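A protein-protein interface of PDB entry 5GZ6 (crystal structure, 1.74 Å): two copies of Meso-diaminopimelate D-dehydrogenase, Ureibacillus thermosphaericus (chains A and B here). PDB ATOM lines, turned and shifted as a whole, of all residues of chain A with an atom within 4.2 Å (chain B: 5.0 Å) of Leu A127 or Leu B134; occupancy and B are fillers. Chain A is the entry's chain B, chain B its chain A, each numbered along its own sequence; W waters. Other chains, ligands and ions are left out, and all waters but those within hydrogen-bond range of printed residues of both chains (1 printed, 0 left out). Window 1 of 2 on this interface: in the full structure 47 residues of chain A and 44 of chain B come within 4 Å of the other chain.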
ATOM      1  N   GLY A 122     -10.707  13.953  11.170  1.00  0.00           N
ATOM      2  CA  GLY A 122     -10.910  12.761  10.371  1.00  0.00           C
ATOM      3  C   GLY A 122      -9.614  12.082   9.976  1.00  0.00           C
ATOM      4  O   GLY A 122      -8.561  12.375  10.535  1.00  0.00           O
ATOM      5  N   TRP A 123      -9.700  11.144   9.040  1.00  0.00           N
ATOM      6  CA  TRP A 123      -8.525  10.427   8.562  1.00  0.00           C
ATOM      7  C   TRP A 123      -7.549  11.324   7.779  1.00  0.00           C
ATOM      8  O   TRP A 123      -6.357  11.351   8.059  1.00  0.00           O
ATOM      9  CB  TRP A 123      -9.018   9.243   7.728  1.00  0.00           C
ATOM     10  CG  TRP A 123      -8.011   8.556   6.902  1.00  0.00           C
ATOM     11  CD1 TRP A 123      -6.659   8.612   7.031  1.00  0.00           C
ATOM     12  CD2 TRP A 123      -8.278   7.656   5.827  1.00  0.00           C
ATOM     13  NE1 TRP A 123      -6.063   7.819   6.085  1.00  0.00           N
ATOM     14  CE2 TRP A 123      -7.037   7.220   5.332  1.00  0.00           C
ATOM     15  CE3 TRP A 123      -9.448   7.186   5.225  1.00  0.00           C
ATOM     16  CZ2 TRP A 123      -6.932   6.335   4.265  1.00  0.00           C
ATOM     17  CZ3 TRP A 123      -9.341   6.308   4.170  1.00  0.00           C
ATOM     18  CH2 TRP A 123      -8.094   5.891   3.699  1.00  0.00           C
ATOM     19  N   PRO A 125      -8.253  15.279   5.920  1.00  0.00           N
ATOM     20  CA  PRO A 125      -7.378  15.779   6.984  1.00  0.00           C
ATOM     21  C   PRO A 125      -7.667  15.162   8.343  1.00  0.00           C
ATOM     22  O   PRO A 125      -8.698  14.525   8.539  1.00  0.00           O
ATOM     23  CB  PRO A 125      -7.692  17.277   7.016  1.00  0.00           C
ATOM     24  CG  PRO A 125      -9.059  17.395   6.437  1.00  0.00           C
ATOM     25  CD  PRO A 125      -9.136  16.328   5.388  1.00  0.00           C
ATOM     26  N   GLY A 126      -6.732  15.338   9.268  1.00  0.00           N
ATOM     27  CA  GLY A 126      -6.868  14.772  10.591  1.00  0.00           C
ATOM     28  C   GLY A 126      -5.646  13.956  10.941  1.00  0.00           C
ATOM     29  O   GLY A 126      -4.569  14.505  11.144  1.00  0.00           O
ATOM     30  N   LEU A 127      -5.809  12.645  11.013  1.00  0.00           N
ATOM     31  CA  LEU A 127      -4.701  11.778  11.373  1.00  0.00           C
ATOM     32  C   LEU A 127      -3.538  11.900  10.398  1.00  0.00           C
ATOM     33  O   LEU A 127      -2.386  11.918  10.815  1.00  0.00           O
ATOM     34  CB  LEU A 127      -5.165  10.324  11.422  1.00  0.00           C
ATOM     35  CG  LEU A 127      -4.059   9.296  11.655  1.00  0.00           C
ATOM     36  CD1 LEU A 127      -3.439   9.501  13.027  1.00  0.00           C
ATOM     37  CD2 LEU A 127      -4.597   7.884  11.512  1.00  0.00           C
ATOM     38  N   PHE A 128      -3.835  11.942   9.110  1.00  0.00           N
ATOM     39  CA  PHE A 128      -2.780  12.058   8.115  1.00  0.00           C
ATOM     40  C   PHE A 128      -2.032  13.382   8.232  1.00  0.00           C
ATOM     41  O   PHE A 128      -0.829  13.443   8.000  1.00  0.00           O
ATOM     42  CB  PHE A 128      -3.274  11.723   6.710  1.00  0.00           C
ATOM     43  CG  PHE A 128      -3.211  10.254   6.400  1.00  0.00           C
ATOM     44  CD1 PHE A 128      -3.214   9.323   7.424  1.00  0.00           C
ATOM     45  CD2 PHE A 128      -3.152   9.803   5.096  1.00  0.00           C
ATOM     46  CE1 PHE A 128      -3.152   7.970   7.155  1.00  0.00           C
ATOM     47  CE2 PHE A 128      -3.091   8.453   4.819  1.00  0.00           C
ATOM     48  CZ  PHE A 128      -3.090   7.534   5.849  1.00  0.00           C
ATOM     49  N   SER A 129      -2.757  14.439   8.580  1.00  0.00           N
ATOM     50  CA  SER A 129      -2.144  15.746   8.748  1.00  0.00           C
ATOM     51  C   SER A 129      -1.125  15.654   9.878  1.00  0.00           C
ATOM     52  O   SER A 129      -0.026  16.188   9.783  1.00  0.00           O
ATOM     53  CB  SER A 129      -3.204  16.789   9.099  1.00  0.00           C
ATOM     54  OG  SER A 129      -4.325  16.681   8.246  1.00  0.00           O
ATOM     55  N   LEU A 130      -1.502  14.958  10.945  1.00  0.00           N
ATOM     56  CA  LEU A 130      -0.615  14.773  12.082  1.00  0.00           C
ATOM     57  C   LEU A 130       0.613  13.982  11.642  1.00  0.00           C
ATOM     58  O   LEU A 130       1.733  14.292  12.033  1.00  0.00           O
ATOM     59  CB  LEU A 130      -1.345  14.066  13.227  1.00  0.00           C
ATOM     60  CG  LEU A 130      -2.482  14.857  13.879  1.00  0.00           C
ATOM     61  CD1 LEU A 130      -3.275  13.992  14.842  1.00  0.00           C
ATOM     62  CD2 LEU A 130      -1.967  16.105  14.578  1.00  0.00           C
ATOM     63  N   ASN A 131       0.398  12.963  10.815  1.00  0.00           N
ATOM     64  CA  ASN A 131       1.513  12.142  10.314  1.00  0.00           C
ATOM     65  C   ASN A 131       2.503  13.039   9.492  1.00  0.00           C
ATOM     66  O   ASN A 131       3.716  12.867   9.613  1.00  0.00           O
ATOM     67  CB  ASN A 131       1.023  11.027   9.439  1.00  0.00           C
ATOM     68  CG  ASN A 131       0.372   9.873  10.211  1.00  0.00           C
ATOM     69  OD1 ASN A 131      -0.395   9.065   9.614  1.00  0.00           O
ATOM     70  ND2 ASN A 131       0.653   9.766  11.431  1.00  0.00           N
ATOM     71  N   LEU A 271      -2.241   3.601   8.139  1.00  0.00           N
ATOM     72  CA  LEU A 271      -3.586   3.331   8.725  1.00  0.00           C
ATOM     73  C   LEU A 271      -4.272   2.325   7.856  1.00  0.00           C
ATOM     74  O   LEU A 271      -4.282   2.469   6.653  1.00  0.00           O
ATOM     75  CB  LEU A 271      -4.435   4.582   8.691  1.00  0.00           C
ATOM     76  CG  LEU A 271      -5.810   4.401   9.312  1.00  0.00           C
ATOM     77  CD1 LEU A 271      -5.647   4.100  10.757  1.00  0.00           C
ATOM     78  CD2 LEU A 271      -6.604   5.646   9.026  1.00  0.00           C
ATOM     79  N   PHE A 310      -4.074  15.084  22.727  1.00  0.00           N
ATOM     80  CA  PHE A 310      -4.848  13.852  22.624  1.00  0.00           C
ATOM     81  C   PHE A 310      -5.578  13.446  23.898  1.00  0.00           C
ATOM     82  O   PHE A 310      -6.560  12.755  23.808  1.00  0.00           O
ATOM     83  CB  PHE A 310      -4.007  12.690  22.192  1.00  0.00           C
ATOM     84  CG  PHE A 310      -3.984  12.433  20.677  1.00  0.00           C
ATOM     85  CD1 PHE A 310      -4.153  13.453  19.758  1.00  0.00           C
ATOM     86  CD2 PHE A 310      -3.756  11.130  20.212  1.00  0.00           C
ATOM     87  CE1 PHE A 310      -4.140  13.196  18.424  1.00  0.00           C
ATOM     88  CE2 PHE A 310      -3.772  10.846  18.881  1.00  0.00           C
ATOM     89  CZ  PHE A 310      -3.946  11.903  17.974  1.00  0.00           C
ATOM     90  N   LEU B 130       0.128   7.224  21.650  1.00  0.00           N
ATOM     91  CA  LEU B 130      -0.882   8.044  20.997  1.00  0.00           C
ATOM     92  C   LEU B 130      -1.825   7.153  20.192  1.00  0.00           C
ATOM     93  O   LEU B 130      -3.028   7.378  20.166  1.00  0.00           O
ATOM     94  CB  LEU B 130      -0.238   9.099  20.098  1.00  0.00           C
ATOM     95  CG  LEU B 130       0.508  10.227  20.813  1.00  0.00           C
ATOM     96  CD1 LEU B 130       1.174  11.159  19.816  1.00  0.00           C
ATOM     97  CD2 LEU B 130      -0.426  10.996  21.730  1.00  0.00           C
ATOM     98  N   ASN B 131      -1.265   6.144  19.533  1.00  0.00           N
ATOM     99  CA  ASN B 131      -2.060   5.215  18.744  1.00  0.00           C
ATOM    100  C   ASN B 131      -3.047   4.428  19.615  1.00  0.00           C
ATOM    101  O   ASN B 131      -4.193   4.224  19.224  1.00  0.00           O
ATOM    102  CB  ASN B 131      -1.159   4.252  17.963  1.00  0.00           C
ATOM    103  CG  ASN B 131      -0.411   4.934  16.829  1.00  0.00           C
ATOM    104  OD1 ASN B 131       0.581   4.411  16.326  1.00  0.00           O
ATOM    105  ND2 ASN B 131      -0.888   6.097  16.419  1.00  0.00           N
ATOM    106  N   ARG B 132      -2.598   3.994  20.793  1.00  0.00           N
ATOM    107  CA  ARG B 132      -3.459   3.241  21.706  1.00  0.00           C
ATOM    108  C   ARG B 132      -4.634   4.110  22.148  1.00  0.00           C
ATOM    109  O   ARG B 132      -5.776   3.666  22.160  1.00  0.00           O
ATOM    110  CB  ARG B 132      -2.663   2.728  22.907  1.00  0.00           C
ATOM    111  CG  ARG B 132      -1.689   1.613  22.558  1.00  0.00           C
ATOM    112  CD  ARG B 132      -1.058   0.992  23.795  1.00  0.00           C
ATOM    113  NE  ARG B 132      -0.014   1.835  24.368  1.00  0.00           N
ATOM    114  CZ  ARG B 132       1.269   1.761  24.037  1.00  0.00           C
ATOM    115  NH1 ARG B 132       1.676   0.880  23.135  1.00  0.00           N
ATOM    116  NH2 ARG B 132       2.150   2.567  24.609  1.00  0.00           N
ATOM    117  N   LEU B 133      -4.343   5.359  22.485  1.00  0.00           N
ATOM    118  CA  LEU B 133      -5.384   6.326  22.838  1.00  0.00           C
ATOM    119  C   LEU B 133      -6.356   6.514  21.740  1.00  0.00           C
ATOM    120  O   LEU B 133      -7.610   6.455  21.930  1.00  0.00           O
ATOM    121  CB  LEU B 133      -4.787   7.597  23.311  1.00  0.00           C
ATOM    122  CG  LEU B 133      -5.743   8.640  23.967  1.00  0.00           C
ATOM    123  CD1 LEU B 133      -4.887   9.526  24.884  1.00  0.00           C
ATOM    124  CD2 LEU B 133      -6.436   9.463  22.951  1.00  0.00           C
ATOM    125  N   LEU B 134      -5.833   6.776  20.536  1.00  0.00           N
ATOM    126  CA  LEU B 134      -6.698   7.054  19.422  1.00  0.00           C
ATOM    127  C   LEU B 134      -7.592   5.817  19.158  1.00  0.00           C
ATOM    128  O   LEU B 134      -8.803   5.972  18.899  1.00  0.00           O
ATOM    129  CB  LEU B 134      -5.887   7.531  18.194  1.00  0.00           C
ATOM    130  CG  LEU B 134      -6.733   7.987  16.977  1.00  0.00           C
ATOM    131  CD1 LEU B 134      -7.502   9.267  17.398  1.00  0.00           C
ATOM    132  CD2 LEU B 134      -5.731   8.376  15.862  1.00  0.00           C
ATOM    133  N   GLY B 135      -7.031   4.623  19.262  1.00  0.00           N
ATOM    134  CA  GLY B 135      -7.824   3.437  19.033  1.00  0.00           C
ATOM    135  C   GLY B 135      -8.962   3.349  20.032  1.00  0.00           C
ATOM    136  O   GLY B 135     -10.079   3.001  19.664  1.00  0.00           O
ATOM    137  N   GLU B 136      -8.686   3.666  21.293  1.00  0.00           N
ATOM    138  CA  GLU B 136      -9.713   3.612  22.333  1.00  0.00           C
ATOM    139  C   GLU B 136     -10.869   4.587  22.146  1.00  0.00           C
ATOM    140  O   GLU B 136     -12.023   4.225  22.344  1.00  0.00           O
ATOM    141  CB  GLU B 136      -9.097   3.857  23.710  1.00  0.00           C
ATOM    142  CG  GLU B 136      -8.350   2.671  24.281  1.00  0.00           C
ATOM    143  CD  GLU B 136      -8.150   2.790  25.775  1.00  0.00           C
ATOM    144  OE1 GLU B 136      -8.482   3.847  26.343  1.00  0.00           O
ATOM    145  OE2 GLU B 136      -7.664   1.821  26.379  1.00  0.00           O
ATOM    146  N   VAL B 137     -10.559   5.828  21.789  1.00  0.00           N
ATOM    147  CA  VAL B 137     -11.598   6.830  21.580  1.00  0.00           C
ATOM    148  C   VAL B 137     -12.469   6.490  20.367  1.00  0.00           C
ATOM    149  O   VAL B 137     -13.679   6.680  20.384  1.00  0.00           O
ATOM    150  CB  VAL B 137     -11.033   8.263  21.521  1.00  0.00           C
ATOM    151  CG1 VAL B 137     -10.368   8.611  22.844  1.00  0.00           C
ATOM    152  CG2 VAL B 137     -10.061   8.419  20.365  1.00  0.00           C
ATOM    153  N   VAL B 138     -11.821   6.009  19.312  1.00  0.00           N
ATOM    154  CA  VAL B 138     -12.489   5.598  18.076  1.00  0.00           C
ATOM    155  C   VAL B 138     -13.388   4.349  18.182  1.00  0.00           C
ATOM    156  O   VAL B 138     -14.445   4.287  17.556  1.00  0.00           O
ATOM    157  CB  VAL B 138     -11.472   5.446  16.918  1.00  0.00           C
ATOM    158  CG1 VAL B 138     -12.120   4.842  15.681  1.00  0.00           C
ATOM    159  CG2 VAL B 138     -10.865   6.796  16.582  1.00  0.00           C
ATOM    160  N   LEU B 139     -12.949   3.356  18.953  1.00  0.00           N
ATOM    161  CA  LEU B 139     -13.637   2.123  19.098  1.00  0.00           C
ATOM    162  C   LEU B 139     -13.625   1.873  20.600  1.00  0.00           C
ATOM    163  O   LEU B 139     -12.741   1.145  21.056  1.00  0.00           O
ATOM    164  CB  LEU B 139     -12.897   0.973  18.383  1.00  0.00           C
ATOM    165  CG  LEU B 139     -13.164   0.731  16.917  1.00  0.00           C
ATOM    166  CD1 LEU B 139     -12.324  -0.476  16.437  1.00  0.00           C
ATOM    167  CD2 LEU B 139     -14.707   0.549  16.675  1.00  0.00           C
ATOM    168  N   PHE B 269      -2.773   0.888  13.205  1.00  0.00           N
ATOM    169  CA  PHE B 269      -1.859   2.077  13.039  1.00  0.00           C
ATOM    170  C   PHE B 269      -0.412   1.559  13.011  1.00  0.00           C
ATOM    171  O   PHE B 269       0.047   0.919  13.929  1.00  0.00           O
ATOM    172  CB  PHE B 269      -1.953   3.002  14.226  1.00  0.00           C
ATOM    173  CG  PHE B 269      -3.298   3.517  14.595  1.00  0.00           C
ATOM    174  CD1 PHE B 269      -3.794   4.642  14.029  1.00  0.00           C
ATOM    175  CD2 PHE B 269      -4.042   2.916  15.604  1.00  0.00           C
ATOM    176  CE1 PHE B 269      -5.032   5.124  14.414  1.00  0.00           C
ATOM    177  CE2 PHE B 269      -5.287   3.328  15.964  1.00  0.00           C
ATOM    178  CZ  PHE B 269      -5.779   4.498  15.404  1.00  0.00           C
HETATM  179  O   HOH W   1       0.101   7.130  13.238  1.00  0.00           O
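The backbone NH (N) of Leu A127 is in hydrogen-bond range of the backbone carbonyl oxygen (O) of Gly A122 (2.8 Å).
CD1 of Leu A127 touches CD2 of Leu B134, 3.8 Å away.
CD1 of Leu A271 touches CD1 of Phe B269, 3.8 Å away.
Leu B130 touches Phe A310.
Phe A310 touches Leu B133.
Leu B134 touches Phe A310.
Of the printed residues of chain A, Leu B134 touches Leu A127 and Phe A310.
Of the printed residues of chain A, Leu B130 touches Phe A310 (3.7 Å).
Printed residues of chain A within 4 Å of Phe B269: Leu A271.
Printed residues of chain B within 4 Å of Leu A271: Phe B269.
Printed residues of chain A within 4 Å of Leu B133: Phe A310.
Of the printed residues of chain B, Phe A310 touches Leu B130, Leu B133 and Leu B134.
Gly A126 touches none of the printed residues of chain B.
The nearest printed residue of chain A that does not touch Leu B134 is Leu A130 (6.2 Å).
Of the 11 printed residues of chain A, 3 touch a printed residue of chain B.
Printed residues of chain A that touch a printed residue of chain B: Leu A127, Leu A271 and Phe A310.
Of the 11 printed residues of chain B, 4 touch a printed residue of chain A.
Printed residues of chain B that touch a printed residue of chain A: Leu B130, Leu B133, Leu B134 and Phe B269.
Hydrophobic or aromatic side chains of chain B that line the printed part of chain A: Leu B130, Leu B133, Leu B134 and Phe B269.
Among the printed residues, no Asp or Glu carboxylate lies within 4 Å of a Lys or Arg side-chain nitrogen of the other chain.
2 positions are printed for both chains.
Of the 5 pairs that touch across the chains among the printed residues, none has its exchanged pair printed and touching as well.
Water W1 lies within hydrogen-bond range of the side-chain amide nitrogen of Asn A131 (3.2 Å) and the side-chain amide nitrogen of Asn B131 (3.5 Å).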
